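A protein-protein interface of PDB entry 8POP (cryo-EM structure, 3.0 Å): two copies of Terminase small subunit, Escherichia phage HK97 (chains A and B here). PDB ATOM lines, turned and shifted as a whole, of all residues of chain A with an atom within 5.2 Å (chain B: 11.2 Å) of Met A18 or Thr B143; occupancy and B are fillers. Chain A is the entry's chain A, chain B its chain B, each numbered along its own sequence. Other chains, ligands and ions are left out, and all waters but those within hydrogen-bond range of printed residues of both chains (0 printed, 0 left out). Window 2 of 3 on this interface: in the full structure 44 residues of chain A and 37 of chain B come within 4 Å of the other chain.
The side-chain hydroxyl (OG1) of Thr B143 sits close to the side-chain sulfur (SD) of Met A18, 3.5 Å away.
The backbone carbonyl oxygen (O) of Ala A21 lies within hydrogen-bond range of the side-chain amino group (NZ) of Lys B144 (3.1 Å).
The backbone carbonyl oxygen (O) of Ala A22 sits at hydrogen-bond distance from the side-chain amino group (NZ) of Lys B144 (3.3 Å).
The side-chain amide nitrogen of Asn A20 sits at hydrogen-bond distance from the side-chain carboxylate of Asp B137 (2.9 Å).
The side-chain amide nitrogen (ND2) of Asn B145 lies within hydrogen-bond range of the backbone carbonyl oxygen (O) of Arg B141 (3.0 Å).
The backbone carbonyl oxygen (O) of Ala B140 is in hydrogen-bond range of the side-chain hydroxyl (OG1) of Thr B143, at 2.5 Å.
The side-chain amide nitrogen (NE2) of Gln A16 sits at hydrogen-bond distance from the side-chain amide oxygen (OD1) of Asn A20.
Among the printed residues, merely in contact across the chains: Ala A17 with Ala B140 (3.4 Å), Met A18 with Ala B140 (3.7 Å), Ala A17 with Asn B136 (3.8 Å) and Ala A21 with Arg B141 (3.8 Å).
Met A18 touches just these residues of chain B: Ala B140 (3.7 Å) and Thr B143 (3.4 Å).
Of chain A, only Met A18 (3.4 Å) comes within 4 Å of Thr B143.
No residue of chain B comes within 4 Å of Val A15.
Ala A17 touches two residues of chain B.
Asn A20 touches just one residue of chain B: Asp B137.
Of chain B, only Arg B141 (3.8 Å) and Lys B144 (3.1 Å) come within 4 Å of Ala A21.
Of chain B, only Lys B144 comes within 4 Å of Ala A22.
Of the printed residues of chain A, Ala B140 touches Ala A17 and Met A18.
Of the printed residues of chain A, Lys B144 touches Ala A21 (3.1 Å) and Ala A22 (3.3 Å).
Printed residues of chain A within 4 Å of Arg B141: Ala A21.
Of the printed residues of chain A, Asp B137 touches Asn A20 (2.9 Å).
Lys A19 touches none of the printed residues of chain B.
The nearest residue of chain B that does not touch Met A18 is Asp B139 (5.5 Å).
The nearest printed residue of chain A that does not touch Ala B140 is Ala A21 (4.2 Å).
Of the 9 printed residues of chain A, 5 touch a printed residue of chain B.
Printed residues of chain A that touch a printed residue of chain B: Ala A17, Met A18, Asn A20, Ala A21 and Ala A22.
Hydrophobic or aromatic side chains of chain A that line the printed part of chain B: Ala A17, Met A18 and Ala A21.
Along chain B the printed residues that touch a printed residue of chain A span positions 136 to 144.
Among the printed residues, 8 pairs touch across the chains.
Among the printed residues, no Asp or Glu carboxylate lies within 4 Å of a Lys or Arg side-chain nitrogen of the other chain.
No position is printed for both chains.
Of the 8 pairs that touch across the chains among the printed residues, none has its exchanged pair printed and touching as well.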
ATOM      1  N   ALA A  14      31.616 -18.855   5.186  1.00  0.00           N
ATOM      2  CA  ALA A  14      31.389 -17.871   6.230  1.00  0.00           C
ATOM      3  C   ALA A  14      29.968 -17.312   6.167  1.00  0.00           C
ATOM      4  O   ALA A  14      29.479 -16.776   7.158  1.00  0.00           O
ATOM      5  CB  ALA A  14      32.393 -16.756   6.102  1.00  0.00           C
ATOM      6  N   VAL A  15      29.333 -17.383   4.990  1.00  0.00           N
ATOM      7  CA  VAL A  15      27.952 -16.947   4.852  1.00  0.00           C
ATOM      8  C   VAL A  15      27.071 -17.919   5.631  1.00  0.00           C
ATOM      9  O   VAL A  15      26.346 -17.523   6.543  1.00  0.00           O
ATOM     10  CB  VAL A  15      27.532 -16.854   3.372  1.00  0.00           C
ATOM     11  CG1 VAL A  15      26.026 -16.698   3.211  1.00  0.00           C
ATOM     12  CG2 VAL A  15      28.262 -15.733   2.653  1.00  0.00           C
ATOM     13  N   GLN A  16      27.165 -19.197   5.247  1.00  0.00           N
ATOM     14  CA  GLN A  16      26.380 -20.277   5.827  1.00  0.00           C
ATOM     15  C   GLN A  16      26.515 -20.277   7.347  1.00  0.00           C
ATOM     16  O   GLN A  16      25.535 -20.475   8.059  1.00  0.00           O
ATOM     17  CB  GLN A  16      26.856 -21.596   5.230  1.00  0.00           C
ATOM     18  CG  GLN A  16      26.098 -22.800   5.730  1.00  0.00           C
ATOM     19  CD  GLN A  16      24.671 -22.778   5.256  1.00  0.00           C
ATOM     20  OE1 GLN A  16      24.406 -22.755   4.058  1.00  0.00           O
ATOM     21  NE2 GLN A  16      23.737 -22.807   6.195  1.00  0.00           N
ATOM     22  N   ALA A  17      27.723 -20.015   7.847  1.00  0.00           N
ATOM     23  CA  ALA A  17      27.899 -19.931   9.284  1.00  0.00           C
ATOM     24  C   ALA A  17      26.999 -18.863   9.898  1.00  0.00           C
ATOM     25  O   ALA A  17      26.387 -19.132  10.924  1.00  0.00           O
ATOM     26  CB  ALA A  17      29.333 -19.688   9.640  1.00  0.00           C
ATOM     27  N   MET A  18      26.926 -17.671   9.278  1.00  0.00           N
ATOM     28  CA  MET A  18      26.169 -16.540   9.811  1.00  0.00           C
ATOM     29  C   MET A  18      24.676 -16.776   9.620  1.00  0.00           C
ATOM     30  O   MET A  18      23.864 -16.403  10.470  1.00  0.00           O
ATOM     31  CB  MET A  18      26.546 -15.238   9.106  1.00  0.00           C
ATOM     32  CG  MET A  18      27.949 -14.781   9.441  1.00  0.00           C
ATOM     33  SD  MET A  18      28.207 -14.418  11.209  1.00  0.00           S
ATOM     34  CE  MET A  18      29.940 -13.950  11.178  1.00  0.00           C
ATOM     35  N   LYS A  19      24.340 -17.389   8.483  1.00  0.00           N
ATOM     36  CA  LYS A  19      22.993 -17.850   8.215  1.00  0.00           C
ATOM     37  C   LYS A  19      22.575 -18.847   9.296  1.00  0.00           C
ATOM     38  O   LYS A  19      21.446 -18.800   9.786  1.00  0.00           O
ATOM     39  CB  LYS A  19      22.959 -18.433   6.800  1.00  0.00           C
ATOM     40  CG  LYS A  19      21.621 -19.029   6.395  1.00  0.00           C
ATOM     41  CD  LYS A  19      21.625 -19.703   5.042  1.00  0.00           C
ATOM     42  CE  LYS A  19      20.436 -20.628   4.874  1.00  0.00           C
ATOM     43  NZ  LYS A  19      20.492 -21.378   3.596  1.00  0.00           N
ATOM     44  N   ASN A  20      23.512 -19.732   9.668  1.00  0.00           N
ATOM     45  CA  ASN A  20      23.271 -20.777  10.654  1.00  0.00           C
ATOM     46  C   ASN A  20      22.917 -20.165  11.995  1.00  0.00           C
ATOM     47  O   ASN A  20      21.848 -20.441  12.507  1.00  0.00           O
ATOM     48  CB  ASN A  20      24.462 -21.722  10.825  1.00  0.00           C
ATOM     49  CG  ASN A  20      24.449 -22.841   9.804  1.00  0.00           C
ATOM     50  OD1 ASN A  20      23.510 -22.935   9.008  1.00  0.00           O
ATOM     51  ND2 ASN A  20      25.470 -23.691   9.819  1.00  0.00           N
ATOM     52  N   ALA A  21      23.785 -19.306  12.528  1.00  0.00           N
ATOM     53  CA  ALA A  21      23.633 -18.810  13.888  1.00  0.00           C
ATOM     54  C   ALA A  21      22.394 -17.929  14.043  1.00  0.00           C
ATOM     55  O   ALA A  21      21.995 -17.656  15.175  1.00  0.00           O
ATOM     56  CB  ALA A  21      24.872 -18.061  14.311  1.00  0.00           C
ATOM     57  N   ALA A  22      21.805 -17.485  12.920  1.00  0.00           N
ATOM     58  CA  ALA A  22      20.562 -16.724  12.937  1.00  0.00           C
ATOM     59  C   ALA A  22      19.408 -17.614  13.389  1.00  0.00           C
ATOM     60  O   ALA A  22      18.752 -17.305  14.379  1.00  0.00           O
ATOM     61  CB  ALA A  22      20.296 -16.121  11.578  1.00  0.00           C
ATOM     62  N   ARG B 133      34.753 -26.821  10.062  1.00  0.00           N
ATOM     63  CA  ARG B 133      33.349 -26.539   9.824  1.00  0.00           C
ATOM     64  C   ARG B 133      32.713 -26.053  11.113  1.00  0.00           C
ATOM     65  O   ARG B 133      32.107 -25.002  11.158  1.00  0.00           O
ATOM     66  CB  ARG B 133      32.700 -27.828   9.337  1.00  0.00           C
ATOM     67  CG  ARG B 133      31.222 -27.756   9.005  1.00  0.00           C
ATOM     68  CD  ARG B 133      30.924 -29.047   8.264  1.00  0.00           C
ATOM     69  NE  ARG B 133      29.559 -29.112   7.785  1.00  0.00           N
ATOM     70  CZ  ARG B 133      29.058 -30.123   7.089  1.00  0.00           C
ATOM     71  NH1 ARG B 133      29.830 -31.145   6.759  1.00  0.00           N
ATOM     72  NH2 ARG B 133      27.788 -30.093   6.714  1.00  0.00           N
ATOM     73  N   ASN B 134      32.910 -26.806  12.177  1.00  0.00           N
ATOM     74  CA  ASN B 134      32.259 -26.501  13.426  1.00  0.00           C
ATOM     75  C   ASN B 134      32.812 -25.224  14.033  1.00  0.00           C
ATOM     76  O   ASN B 134      32.055 -24.467  14.632  1.00  0.00           O
ATOM     77  CB  ASN B 134      32.405 -27.653  14.414  1.00  0.00           C
ATOM     78  CG  ASN B 134      31.429 -28.777  14.136  1.00  0.00           C
ATOM     79  OD1 ASN B 134      30.220 -28.540  14.033  1.00  0.00           O
ATOM     80  ND2 ASN B 134      31.948 -29.994  14.057  1.00  0.00           N
ATOM     81  N   GLN B 135      34.128 -25.023  13.929  1.00  0.00           N
ATOM     82  CA  GLN B 135      34.786 -23.867  14.514  1.00  0.00           C
ATOM     83  C   GLN B 135      34.136 -22.600  13.999  1.00  0.00           C
ATOM     84  O   GLN B 135      33.813 -21.717  14.789  1.00  0.00           O
ATOM     85  CB  GLN B 135      36.251 -23.811  14.100  1.00  0.00           C
ATOM     86  CG  GLN B 135      37.021 -22.657  14.716  1.00  0.00           C
ATOM     87  CD  GLN B 135      37.060 -22.728  16.223  1.00  0.00           C
ATOM     88  OE1 GLN B 135      37.297 -23.783  16.806  1.00  0.00           O
ATOM     89  NE2 GLN B 135      36.835 -21.595  16.872  1.00  0.00           N
ATOM     90  N   ASN B 136      33.949 -22.548  12.672  1.00  0.00           N
ATOM     91  CA  ASN B 136      33.385 -21.385  12.001  1.00  0.00           C
ATOM     92  C   ASN B 136      32.005 -21.063  12.553  1.00  0.00           C
ATOM     93  O   ASN B 136      31.637 -19.899  12.662  1.00  0.00           O
ATOM     94  CB  ASN B 136      33.228 -21.599  10.496  1.00  0.00           C
ATOM     95  CG  ASN B 136      34.552 -21.678   9.774  1.00  0.00           C
ATOM     96  OD1 ASN B 136      35.573 -21.211  10.281  1.00  0.00           O
ATOM     97  ND2 ASN B 136      34.533 -22.237   8.577  1.00  0.00           N
ATOM     98  N   ASP B 137      31.241 -22.102  12.875  1.00  0.00           N
ATOM     99  CA  ASP B 137      29.923 -21.909  13.438  1.00  0.00           C
ATOM    100  C   ASP B 137      30.042 -21.325  14.838  1.00  0.00           C
ATOM    101  O   ASP B 137      29.362 -20.364  15.177  1.00  0.00           O
ATOM    102  CB  ASP B 137      29.136 -23.216  13.415  1.00  0.00           C
ATOM    103  CG  ASP B 137      28.526 -23.539  12.053  1.00  0.00           C
ATOM    104  OD1 ASP B 137      29.274 -23.565  11.035  1.00  0.00           O
ATOM    105  OD2 ASP B 137      27.295 -23.764  12.014  1.00  0.00           O
ATOM    106  N   ARG B 138      30.907 -21.897  15.659  1.00  0.00           N
ATOM    107  CA  ARG B 138      31.135 -21.332  16.977  1.00  0.00           C
ATOM    108  C   ARG B 138      31.472 -19.844  16.852  1.00  0.00           C
ATOM    109  O   ARG B 138      31.052 -19.045  17.689  1.00  0.00           O
ATOM    110  CB  ARG B 138      32.223 -22.117  17.730  1.00  0.00           C
ATOM    111  CG  ARG B 138      31.668 -23.236  18.602  1.00  0.00           C
ATOM    112  CD  ARG B 138      32.635 -23.830  19.610  1.00  0.00           C
ATOM    113  NE  ARG B 138      33.950 -24.106  19.056  1.00  0.00           N
ATOM    114  CZ  ARG B 138      34.309 -25.254  18.480  1.00  0.00           C
ATOM    115  NH1 ARG B 138      35.585 -25.476  18.214  1.00  0.00           N
ATOM    116  NH2 ARG B 138      33.410 -26.186  18.191  1.00  0.00           N
ATOM    117  N   ASP B 139      32.249 -19.485  15.820  1.00  0.00           N
ATOM    118  CA  ASP B 139      32.706 -18.115  15.658  1.00  0.00           C
ATOM    119  C   ASP B 139      31.516 -17.219  15.322  1.00  0.00           C
ATOM    120  O   ASP B 139      31.189 -16.316  16.094  1.00  0.00           O
ATOM    121  CB  ASP B 139      33.863 -18.033  14.661  1.00  0.00           C
ATOM    122  CG  ASP B 139      35.236 -18.241  15.299  1.00  0.00           C
ATOM    123  OD1 ASP B 139      35.313 -18.319  16.553  1.00  0.00           O
ATOM    124  OD2 ASP B 139      36.234 -18.321  14.541  1.00  0.00           O
ATOM    125  N   ALA B 140      30.825 -17.526  14.215  1.00  0.00           N
ATOM    126  CA  ALA B 140      29.566 -16.869  13.878  1.00  0.00           C
ATOM    127  C   ALA B 140      28.732 -16.623  15.134  1.00  0.00           C
ATOM    128  O   ALA B 140      28.335 -15.494  15.395  1.00  0.00           O
ATOM    129  CB  ALA B 140      28.787 -17.670  12.853  1.00  0.00           C
ATOM    130  N   ARG B 141      28.511 -17.678  15.920  1.00  0.00           N
ATOM    131  CA  ARG B 141      27.670 -17.606  17.104  1.00  0.00           C
ATOM    132  C   ARG B 141      28.168 -16.598  18.149  1.00  0.00           C
ATOM    133  O   ARG B 141      27.452 -16.321  19.109  1.00  0.00           O
ATOM    134  CB  ARG B 141      27.572 -18.981  17.774  1.00  0.00           C
ATOM    135  CG  ARG B 141      26.415 -19.849  17.299  1.00  0.00           C
ATOM    136  CD  ARG B 141      25.881 -20.684  18.462  1.00  0.00           C
ATOM    137  NE  ARG B 141      24.600 -21.306  18.166  1.00  0.00           N
ATOM    138  CZ  ARG B 141      24.435 -22.242  17.247  1.00  0.00           C
ATOM    139  NH1 ARG B 141      25.495 -22.804  16.685  1.00  0.00           N
ATOM    140  NH2 ARG B 141      23.216 -22.633  16.910  1.00  0.00           N
ATOM    141  N   ASN B 142      29.401 -16.103  18.034  1.00  0.00           N
ATOM    142  CA  ASN B 142      29.869 -15.114  18.988  1.00  0.00           C
ATOM    143  C   ASN B 142      29.605 -13.725  18.417  1.00  0.00           C
ATOM    144  O   ASN B 142      29.071 -12.859  19.106  1.00  0.00           O
ATOM    145  CB  ASN B 142      31.335 -15.326  19.365  1.00  0.00           C
ATOM    146  CG  ASN B 142      31.519 -16.472  20.337  1.00  0.00           C
ATOM    147  OD1 ASN B 142      31.642 -16.251  21.539  1.00  0.00           O
ATOM    148  ND2 ASN B 142      31.505 -17.698  19.836  1.00  0.00           N
ATOM    149  N   THR B 143      29.976 -13.537  17.146  1.00  0.00           N
ATOM    150  CA  THR B 143      29.765 -12.276  16.456  1.00  0.00           C
ATOM    151  C   THR B 143      28.332 -11.801  16.669  1.00  0.00           C
ATOM    152  O   THR B 143      28.092 -10.603  16.803  1.00  0.00           O
ATOM    153  CB  THR B 143      30.045 -12.398  14.953  1.00  0.00           C
ATOM    154  OG1 THR B 143      29.139 -13.354  14.394  1.00  0.00           O
ATOM    155  CG2 THR B 143      31.475 -12.790  14.651  1.00  0.00           C
ATOM    156  N   LYS B 144      27.392 -12.753  16.686  1.00  0.00           N
ATOM    157  CA  LYS B 144      25.989 -12.450  16.907  1.00  0.00           C
ATOM    158  C   LYS B 144      25.812 -11.821  18.289  1.00  0.00           C
ATOM    159  O   LYS B 144      25.328 -10.695  18.399  1.00  0.00           O
ATOM    160  CB  LYS B 144      25.129 -13.708  16.742  1.00  0.00           C
ATOM    161  CG  LYS B 144      23.644 -13.423  16.576  1.00  0.00           C
ATOM    162  CD  LYS B 144      22.748 -14.640  16.532  1.00  0.00           C
ATOM    163  CE  LYS B 144      21.300 -14.257  16.295  1.00  0.00           C
ATOM    164  NZ  LYS B 144      20.375 -15.381  16.572  1.00  0.00           N
ATOM    165  N   ASN B 145      26.229 -12.549  19.334  1.00  0.00           N
ATOM    166  CA  ASN B 145      26.052 -12.110  20.710  1.00  0.00           C
ATOM    167  C   ASN B 145      26.926 -10.874  20.968  1.00  0.00           C
ATOM    168  O   ASN B 145      26.419  -9.934  21.617  1.00  0.00           O
ATOM    169  CB  ASN B 145      26.372 -13.224  21.713  1.00  0.00           C
ATOM    170  CG  ASN B 145      25.336 -14.330  21.751  1.00  0.00           C
ATOM    171  OD1 ASN B 145      24.646 -14.499  22.755  1.00  0.00           O
ATOM    172  ND2 ASN B 145      25.223 -15.092  20.675  1.00  0.00           N
